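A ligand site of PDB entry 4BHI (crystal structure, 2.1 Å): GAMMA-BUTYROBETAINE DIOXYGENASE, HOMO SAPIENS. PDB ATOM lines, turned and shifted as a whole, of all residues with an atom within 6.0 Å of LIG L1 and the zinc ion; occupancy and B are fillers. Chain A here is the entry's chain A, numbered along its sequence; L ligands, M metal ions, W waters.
Water W1 lies within hydrogen-bond range of the side-chain hydroxyl of Ser 229 (2.7 Å), an oxygen (O4) of LIG L1 (2.8 Å) and the backbone carbonyl oxygen of Gly 348 (3.2 Å).
The zinc ion is bound by an oxygen (O1) of LIG L1 (2.1 Å), the side-chain carboxylate of Asp 204 (2.1 Å), a ring nitrogen (NE2) of His 202 (2.2 Å), a ring nitrogen (NE2) of His 347 (2.2 Å) and an oxygen (O3) of LIG L1 (2.2 Å).
The zinc ion has five donor atoms within binding distance.
Of the 22 residues printed, 3 come within 4 Å of the zinc ion.
Along chain A the residues within 4 Å of the zinc ion span positions 202 to 347.
NH1 of Arg 349 lies within salt-bridge range of O5 of LIG L1 (2.9 Å).
The guanidinium group of Arg 360 lies within salt-bridge range of an oxygen (O4) of LIG L1 (2.9 Å).
The side-chain amide nitrogen (ND2) of Asn 191 is in hydrogen-bond range of an oxygen (O2) of LG2 L2, at 3.0 Å.
O1 of LG2 L2 is in hydrogen-bond range of ND2 of Asn 292 (3.1 Å).
The side-chain hydroxyl (OH) of Tyr 366 sits close to a nitrogen (N1) of LG2 L2, at 3.3 Å.
Residues that only touch LIG L1: Ala 193, Val 183, Leu 362, Leu 199 and Leu 217.
Hydrophobic or aromatic side chains that line LIG L1: Val 183, Ala 193, Leu 199, His 202, Leu 217, His 347 and Leu 362.
Ten residues have an atom within 4 Å of LIG L1: Val 183, Ala 193, Leu 199, His 202, Asp 204, Leu 217, His 347, Arg 349, Arg 360 and Leu 362.
The side-chain amide nitrogen of Gln 215 lies close to the side-chain carboxylate of Asp 204 (3.3 Å).
OH of Tyr 366 lies within hydrogen-bond range of OD2 of Asp 204 (2.4 Å).
The guanidinium group of Arg 349 is in hydrogen-bond range of the backbone carbonyl oxygen of Ala 193, at 2.9 Å.
N of Leu 199 sits at hydrogen-bond distance from O of Arg 349, at 2.8 Å.
The guanidinium group of Arg 360 lies within hydrogen-bond range of the backbone carbonyl oxygen of Gly 227, 3.0 Å away.
The backbone NH (N) of Ala 193 lies within hydrogen-bond range of the side-chain amide oxygen (OD1) of Asn 191 (3.0 Å).
The backbone NH of Val 183 is in hydrogen-bond range of the backbone carbonyl oxygen of Leu 362, at 2.7 Å.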
ATOM      1  N   TRP A 181       5.507  -7.580 -15.289  1.00  0.00           N
ATOM      2  CA  TRP A 181       4.565  -7.470 -16.399  1.00  0.00           C
ATOM      3  C   TRP A 181       3.455  -6.508 -15.997  1.00  0.00           C
ATOM      4  O   TRP A 181       3.171  -6.329 -14.805  1.00  0.00           O
ATOM      5  CB  TRP A 181       3.975  -8.851 -16.801  1.00  0.00           C
ATOM      6  CG  TRP A 181       3.927  -9.860 -15.686  1.00  0.00           C
ATOM      7  CD1 TRP A 181       4.882 -10.776 -15.401  1.00  0.00           C
ATOM      8  CD2 TRP A 181       2.890 -10.044 -14.728  1.00  0.00           C
ATOM      9  NE1 TRP A 181       4.527 -11.514 -14.304  1.00  0.00           N
ATOM     10  CE2 TRP A 181       3.311 -11.080 -13.868  1.00  0.00           C
ATOM     11  CE3 TRP A 181       1.663  -9.445 -14.507  1.00  0.00           C
ATOM     12  CZ2 TRP A 181       2.532 -11.534 -12.817  1.00  0.00           C
ATOM     13  CZ3 TRP A 181       0.902  -9.886 -13.450  1.00  0.00           C
ATOM     14  CH2 TRP A 181       1.329 -10.936 -12.633  1.00  0.00           C
ATOM     15  N   VAL A 183      -0.389  -5.399 -16.165  1.00  0.00           N
ATOM     16  CA  VAL A 183      -1.760  -5.826 -16.356  1.00  0.00           C
ATOM     17  C   VAL A 183      -2.565  -4.605 -16.747  1.00  0.00           C
ATOM     18  O   VAL A 183      -2.857  -3.747 -15.920  1.00  0.00           O
ATOM     19  CB  VAL A 183      -2.357  -6.486 -15.099  1.00  0.00           C
ATOM     20  CG1 VAL A 183      -3.769  -6.953 -15.358  1.00  0.00           C
ATOM     21  CG2 VAL A 183      -1.500  -7.651 -14.677  1.00  0.00           C
ATOM     22  N   ASN A 191      -2.983 -12.340 -23.983  1.00  0.00           N
ATOM     23  CA  ASN A 191      -3.458 -12.992 -22.765  1.00  0.00           C
ATOM     24  C   ASN A 191      -4.750 -12.320 -22.332  1.00  0.00           C
ATOM     25  O   ASN A 191      -4.851 -11.085 -22.366  1.00  0.00           O
ATOM     26  CB  ASN A 191      -2.381 -12.895 -21.648  1.00  0.00           C
ATOM     27  CG  ASN A 191      -2.609 -13.898 -20.513  1.00  0.00           C
ATOM     28  OD1 ASN A 191      -3.430 -13.671 -19.624  1.00  0.00           O
ATOM     29  ND2 ASN A 191      -1.854 -14.984 -20.517  1.00  0.00           N
ATOM     30  N   ALA A 193      -5.688 -11.773 -19.507  1.00  0.00           N
ATOM     31  CA  ALA A 193      -5.341 -10.824 -18.431  1.00  0.00           C
ATOM     32  C   ALA A 193      -5.228  -9.376 -18.952  1.00  0.00           C
ATOM     33  O   ALA A 193      -5.610  -8.427 -18.266  1.00  0.00           O
ATOM     34  CB  ALA A 193      -4.062 -11.242 -17.732  1.00  0.00           C
ATOM     35  N   TYR A 194      -4.739  -9.227 -20.193  1.00  0.00           N
ATOM     36  CA  TYR A 194      -4.459  -7.921 -20.807  1.00  0.00           C
ATOM     37  C   TYR A 194      -5.648  -7.371 -21.629  1.00  0.00           C
ATOM     38  O   TYR A 194      -5.471  -6.838 -22.749  1.00  0.00           O
ATOM     39  CB  TYR A 194      -3.194  -8.022 -21.683  1.00  0.00           C
ATOM     40  CG  TYR A 194      -1.945  -8.511 -20.931  1.00  0.00           C
ATOM     41  CD1 TYR A 194      -1.794  -8.287 -19.558  1.00  0.00           C
ATOM     42  CD2 TYR A 194      -0.933  -9.200 -21.594  1.00  0.00           C
ATOM     43  CE1 TYR A 194      -0.699  -8.732 -18.877  1.00  0.00           C
ATOM     44  CE2 TYR A 194       0.187  -9.662 -20.901  1.00  0.00           C
ATOM     45  CZ  TYR A 194       0.288  -9.405 -19.551  1.00  0.00           C
ATOM     46  OH  TYR A 194       1.357  -9.807 -18.813  1.00  0.00           O
ATOM     47  N   LEU A 199     -12.019 -11.923 -15.043  1.00  0.00           N
ATOM     48  CA  LEU A 199     -11.241 -13.131 -14.841  1.00  0.00           C
ATOM     49  C   LEU A 199     -11.918 -13.892 -13.723  1.00  0.00           C
ATOM     50  O   LEU A 199     -11.998 -13.406 -12.585  1.00  0.00           O
ATOM     51  CB  LEU A 199      -9.778 -12.808 -14.468  1.00  0.00           C
ATOM     52  CG  LEU A 199      -9.001 -11.934 -15.471  1.00  0.00           C
ATOM     53  CD1 LEU A 199      -7.615 -11.594 -14.985  1.00  0.00           C
ATOM     54  CD2 LEU A 199      -8.872 -12.645 -16.805  1.00  0.00           C
ATOM     55  N   HIS A 202      -8.839 -18.319 -10.832  1.00  0.00           N
ATOM     56  CA  HIS A 202      -7.793 -19.123 -11.409  1.00  0.00           C
ATOM     57  C   HIS A 202      -6.517 -18.990 -10.592  1.00  0.00           C
ATOM     58  O   HIS A 202      -6.406 -18.103  -9.748  1.00  0.00           O
ATOM     59  CB  HIS A 202      -7.500 -18.598 -12.812  1.00  0.00           C
ATOM     60  CG  HIS A 202      -6.946 -17.223 -12.823  1.00  0.00           C
ATOM     61  ND1 HIS A 202      -7.739 -16.110 -12.694  1.00  0.00           N
ATOM     62  CD2 HIS A 202      -5.673 -16.775 -12.873  1.00  0.00           C
ATOM     63  CE1 HIS A 202      -6.969 -15.029 -12.688  1.00  0.00           C
ATOM     64  NE2 HIS A 202      -5.719 -15.408 -12.827  1.00  0.00           N
ATOM     65  N   THR A 203      -5.572 -19.882 -10.864  1.00  0.00           N
ATOM     66  CA  THR A 203      -4.186 -19.722 -10.478  1.00  0.00           C
ATOM     67  C   THR A 203      -3.438 -19.285 -11.725  1.00  0.00           C
ATOM     68  O   THR A 203      -3.860 -19.600 -12.833  1.00  0.00           O
ATOM     69  CB  THR A 203      -3.596 -21.053  -9.973  1.00  0.00           C
ATOM     70  OG1 THR A 203      -3.726 -22.078 -10.984  1.00  0.00           O
ATOM     71  CG2 THR A 203      -4.337 -21.519  -8.720  1.00  0.00           C
ATOM     72  N   ASP A 204      -2.328 -18.564 -11.548  1.00  0.00           N
ATOM     73  CA  ASP A 204      -1.475 -18.152 -12.667  1.00  0.00           C
ATOM     74  C   ASP A 204      -0.539 -19.247 -13.099  1.00  0.00           C
ATOM     75  O   ASP A 204       0.046 -19.943 -12.292  1.00  0.00           O
ATOM     76  CB  ASP A 204      -0.633 -16.920 -12.325  1.00  0.00           C
ATOM     77  CG  ASP A 204      -1.350 -15.625 -12.570  1.00  0.00           C
ATOM     78  OD1 ASP A 204      -2.596 -15.596 -12.444  1.00  0.00           O
ATOM     79  OD2 ASP A 204      -0.652 -14.629 -12.886  1.00  0.00           O
ATOM     80  N   GLN A 215       2.794 -14.709  -5.923  1.00  0.00           N
ATOM     81  CA  GLN A 215       2.507 -13.647  -6.868  1.00  0.00           C
ATOM     82  C   GLN A 215       2.498 -12.322  -6.139  1.00  0.00           C
ATOM     83  O   GLN A 215       2.048 -12.224  -5.005  1.00  0.00           O
ATOM     84  CB  GLN A 215       1.149 -13.873  -7.544  1.00  0.00           C
ATOM     85  CG  GLN A 215       0.864 -12.893  -8.682  1.00  0.00           C
ATOM     86  CD  GLN A 215      -0.436 -13.144  -9.415  1.00  0.00           C
ATOM     87  OE1 GLN A 215      -1.095 -12.202  -9.829  1.00  0.00           O
ATOM     88  NE2 GLN A 215      -0.808 -14.414  -9.598  1.00  0.00           N
ATOM     89  N   LEU A 217       1.303  -8.270  -6.844  1.00  0.00           N
ATOM     90  CA  LEU A 217       0.471  -7.447  -7.719  1.00  0.00           C
ATOM     91  C   LEU A 217       0.300  -6.078  -7.124  1.00  0.00           C
ATOM     92  O   LEU A 217      -0.235  -5.933  -6.036  1.00  0.00           O
ATOM     93  CB  LEU A 217      -0.927  -8.047  -7.911  1.00  0.00           C
ATOM     94  CG  LEU A 217      -1.299  -8.833  -9.174  1.00  0.00           C
ATOM     95  CD1 LEU A 217      -2.811  -9.038  -9.197  1.00  0.00           C
ATOM     96  CD2 LEU A 217      -0.865  -8.115 -10.417  1.00  0.00           C
ATOM     97  N   GLY A 227     -13.347  -3.794 -11.886  1.00  0.00           N
ATOM     98  CA  GLY A 227     -11.969  -4.156 -11.541  1.00  0.00           C
ATOM     99  C   GLY A 227     -11.698  -4.542 -10.101  1.00  0.00           C
ATOM    100  O   GLY A 227     -10.545  -4.574  -9.683  1.00  0.00           O
ATOM    101  N   ASP A 228     -12.754  -4.888  -9.346  1.00  0.00           N
ATOM    102  CA  ASP A 228     -12.584  -5.384  -7.989  1.00  0.00           C
ATOM    103  C   ASP A 228     -11.836  -6.701  -8.065  1.00  0.00           C
ATOM    104  O   ASP A 228     -11.903  -7.381  -9.085  1.00  0.00           O
ATOM    105  CB  ASP A 228     -13.921  -5.643  -7.266  1.00  0.00           C
ATOM    106  CG  ASP A 228     -14.814  -4.429  -7.217  1.00  0.00           C
ATOM    107  OD1 ASP A 228     -15.384  -4.088  -8.264  1.00  0.00           O
ATOM    108  OD2 ASP A 228     -14.961  -3.843  -6.132  1.00  0.00           O
ATOM    109  N   SER A 229     -11.150  -7.034  -6.976  1.00  0.00           N
ATOM    110  CA  SER A 229     -10.427  -8.288  -6.835  1.00  0.00           C
ATOM    111  C   SER A 229     -11.265  -9.253  -5.998  1.00  0.00           C
ATOM    112  O   SER A 229     -12.066  -8.843  -5.129  1.00  0.00           O
ATOM    113  CB  SER A 229      -9.082  -8.043  -6.159  1.00  0.00           C
ATOM    114  OG  SER A 229      -8.317  -7.026  -6.811  1.00  0.00           O
ATOM    115  N   ASN A 292      -6.368 -22.531 -14.626  1.00  0.00           N
ATOM    116  CA  ASN A 292      -6.757 -21.310 -15.306  1.00  0.00           C
ATOM    117  C   ASN A 292      -7.611 -21.719 -16.512  1.00  0.00           C
ATOM    118  O   ASN A 292      -7.197 -22.539 -17.330  1.00  0.00           O
ATOM    119  CB  ASN A 292      -5.530 -20.505 -15.713  1.00  0.00           C
ATOM    120  CG  ASN A 292      -5.882 -19.119 -16.268  1.00  0.00           C
ATOM    121  OD1 ASN A 292      -6.970 -18.897 -16.809  1.00  0.00           O
ATOM    122  ND2 ASN A 292      -4.958 -18.181 -16.141  1.00  0.00           N
ATOM    123  N   MET A 332      -8.448  -2.944  -4.942  1.00  0.00           N
ATOM    124  CA  MET A 332      -7.140  -2.342  -4.755  1.00  0.00           C
ATOM    125  C   MET A 332      -7.167  -0.866  -5.170  1.00  0.00           C
ATOM    126  O   MET A 332      -7.827  -0.492  -6.132  1.00  0.00           O
ATOM    127  CB  MET A 332      -6.096  -3.075  -5.598  1.00  0.00           C
ATOM    128  CG  MET A 332      -5.957  -4.570  -5.312  1.00  0.00           C
ATOM    129  SD  MET A 332      -4.556  -5.304  -6.227  1.00  0.00           S
ATOM    130  CE  MET A 332      -3.204  -4.483  -5.383  1.00  0.00           C
ATOM    131  N   HIS A 347      -7.576 -16.538  -7.670  1.00  0.00           N
ATOM    132  CA  HIS A 347      -7.871 -15.130  -7.670  1.00  0.00           C
ATOM    133  C   HIS A 347      -8.566 -14.772  -8.942  1.00  0.00           C
ATOM    134  O   HIS A 347      -8.553 -15.552  -9.927  1.00  0.00           O
ATOM    135  CB  HIS A 347      -6.608 -14.314  -7.456  1.00  0.00           C
ATOM    136  CG  HIS A 347      -5.597 -14.446  -8.560  1.00  0.00           C
ATOM    137  ND1 HIS A 347      -4.843 -15.595  -8.734  1.00  0.00           N
ATOM    138  CD2 HIS A 347      -5.250 -13.607  -9.554  1.00  0.00           C
ATOM    139  CE1 HIS A 347      -4.055 -15.439  -9.785  1.00  0.00           C
ATOM    140  NE2 HIS A 347      -4.282 -14.238 -10.295  1.00  0.00           N
ATOM    141  N   GLY A 348      -9.233 -13.624  -8.909  1.00  0.00           N
ATOM    142  CA  GLY A 348      -9.914 -13.122 -10.065  1.00  0.00           C
ATOM    143  C   GLY A 348     -10.171 -11.644 -10.053  1.00  0.00           C
ATOM    144  O   GLY A 348      -9.785 -10.913  -9.132  1.00  0.00           O
ATOM    145  N   ARG A 349     -10.863 -11.210 -11.081  1.00  0.00           N
ATOM    146  CA  ARG A 349     -11.057  -9.789 -11.298  1.00  0.00           C
ATOM    147  C   ARG A 349     -12.428  -9.573 -11.943  1.00  0.00           C
ATOM    148  O   ARG A 349     -12.816 -10.326 -12.828  1.00  0.00           O
ATOM    149  CB  ARG A 349      -9.951  -9.286 -12.229  1.00  0.00           C
ATOM    150  CG  ARG A 349     -10.309  -8.017 -12.965  1.00  0.00           C
ATOM    151  CD  ARG A 349      -9.207  -7.630 -13.931  1.00  0.00           C
ATOM    152  NE  ARG A 349      -9.447  -8.099 -15.268  1.00  0.00           N
ATOM    153  CZ  ARG A 349      -8.504  -8.212 -16.204  1.00  0.00           C
ATOM    154  NH1 ARG A 349      -7.240  -7.908 -15.923  1.00  0.00           N
ATOM    155  NH2 ARG A 349      -8.833  -8.638 -17.413  1.00  0.00           N
ATOM    156  N   ARG A 360      -6.598   1.630 -15.985  1.00  0.00           N
ATOM    157  CA  ARG A 360      -6.287   0.593 -15.010  1.00  0.00           C
ATOM    158  C   ARG A 360      -4.976  -0.073 -15.344  1.00  0.00           C
ATOM    159  O   ARG A 360      -4.762  -0.501 -16.488  1.00  0.00           O
ATOM    160  CB  ARG A 360      -7.397  -0.459 -14.987  1.00  0.00           C
ATOM    161  CG  ARG A 360      -7.289  -1.427 -13.815  1.00  0.00           C
ATOM    162  CD  ARG A 360      -8.434  -2.398 -13.803  1.00  0.00           C
ATOM    163  NE  ARG A 360      -8.478  -3.200 -12.570  1.00  0.00           N
ATOM    164  CZ  ARG A 360      -7.838  -4.347 -12.370  1.00  0.00           C
ATOM    165  NH1 ARG A 360      -7.018  -4.871 -13.280  1.00  0.00           N
ATOM    166  NH2 ARG A 360      -8.015  -4.983 -11.219  1.00  0.00           N
ATOM    167  N   LEU A 362      -1.925  -2.558 -13.349  1.00  0.00           N
ATOM    168  CA  LEU A 362      -1.244  -3.258 -12.277  1.00  0.00           C
ATOM    169  C   LEU A 362       0.139  -3.686 -12.786  1.00  0.00           C
ATOM    170  O   LEU A 362       0.308  -3.933 -13.982  1.00  0.00           O
ATOM    171  CB  LEU A 362      -2.059  -4.472 -11.811  1.00  0.00           C
ATOM    172  CG  LEU A 362      -3.552  -4.391 -11.468  1.00  0.00           C
ATOM    173  CD1 LEU A 362      -4.118  -5.780 -11.203  1.00  0.00           C
ATOM    174  CD2 LEU A 362      -3.859  -3.499 -10.273  1.00  0.00           C
ATOM    175  N   TYR A 366       6.418 -12.719 -10.155  1.00  0.00           N
ATOM    176  CA  TYR A 366       6.348 -13.989  -9.485  1.00  0.00           C
ATOM    177  C   TYR A 366       7.598 -14.235  -8.649  1.00  0.00           C
ATOM    178  O   TYR A 366       8.662 -13.696  -8.946  1.00  0.00           O
ATOM    179  CB  TYR A 366       6.234 -15.094 -10.531  1.00  0.00           C
ATOM    180  CG  TYR A 366       4.999 -15.032 -11.402  1.00  0.00           C
ATOM    181  CD1 TYR A 366       3.719 -15.036 -10.843  1.00  0.00           C
ATOM    182  CD2 TYR A 366       5.112 -14.981 -12.784  1.00  0.00           C
ATOM    183  CE1 TYR A 366       2.585 -14.992 -11.638  1.00  0.00           C
ATOM    184  CE2 TYR A 366       3.985 -14.946 -13.600  1.00  0.00           C
ATOM    185  CZ  TYR A 366       2.724 -14.977 -13.022  1.00  0.00           C
ATOM    186  OH  TYR A 366       1.589 -14.933 -13.818  1.00  0.00           O
HETATM  187  C1  LIG L   1      -3.939 -11.809 -14.011  1.00  0.00           C
HETATM  188  C2  LIG L   1      -4.793 -11.405 -12.883  1.00  0.00           C
HETATM  189  C3  LIG L   1      -5.793  -9.587 -11.685  1.00  0.00           C
HETATM  190  C4  LIG L   1      -6.363  -8.243 -12.039  1.00  0.00           C
HETATM  191  O1  LIG L   1      -3.749 -13.036 -14.230  1.00  0.00           O
HETATM  192  O2  LIG L   1      -3.437 -10.883 -14.719  1.00  0.00           O
HETATM  193  O3  LIG L   1      -5.283 -12.240 -12.111  1.00  0.00           O
HETATM  194  O4  LIG L   1      -6.928  -7.708 -11.101  1.00  0.00           O
HETATM  195  N1  LIG L   1      -4.983 -10.105 -12.752  1.00  0.00           N
HETATM  196  O5  LIG L   1      -6.248  -7.741 -13.177  1.00  0.00           O
HETATM  197  O1  LG2 L   2      -1.868 -18.092 -16.483  1.00  0.00           O
HETATM  198  C1  LG2 L   2      -1.992 -17.107 -17.229  1.00  0.00           C
HETATM  199  O2  LG2 L   2      -1.917 -17.216 -18.484  1.00  0.00           O
HETATM  200  C2  LG2 L   2      -2.325 -15.726 -16.660  1.00  0.00           C
HETATM  201  C3  LG2 L   2      -1.291 -15.047 -15.800  1.00  0.00           C
HETATM  202  N1  LG2 L   2      -0.200 -14.451 -16.588  1.00  0.00           N
HETATM  203  C4  LG2 L   2       0.674 -15.464 -17.147  1.00  0.00           C
HETATM  204  N2  LG2 L   2       0.034 -13.095 -16.754  1.00  0.00           N
HETATM  205  C5  LG2 L   2      -0.230 -12.670 -18.142  1.00  0.00           C
HETATM  206  C6  LG2 L   2      -0.771 -12.251 -15.844  1.00  0.00           C
HETATM  207  C7  LG2 L   2       1.442 -12.779 -16.455  1.00  0.00           C
HETATM  208 ZN    ZN M   1      -4.077 -14.044 -12.449  1.00  0.00          ZN
HETATM  209  O   HOH W   1      -7.396  -8.871  -8.620  1.00  0.00           O
HETATM  210  O   HOH W   2      -5.419 -14.766 -16.446  1.00  0.00           O
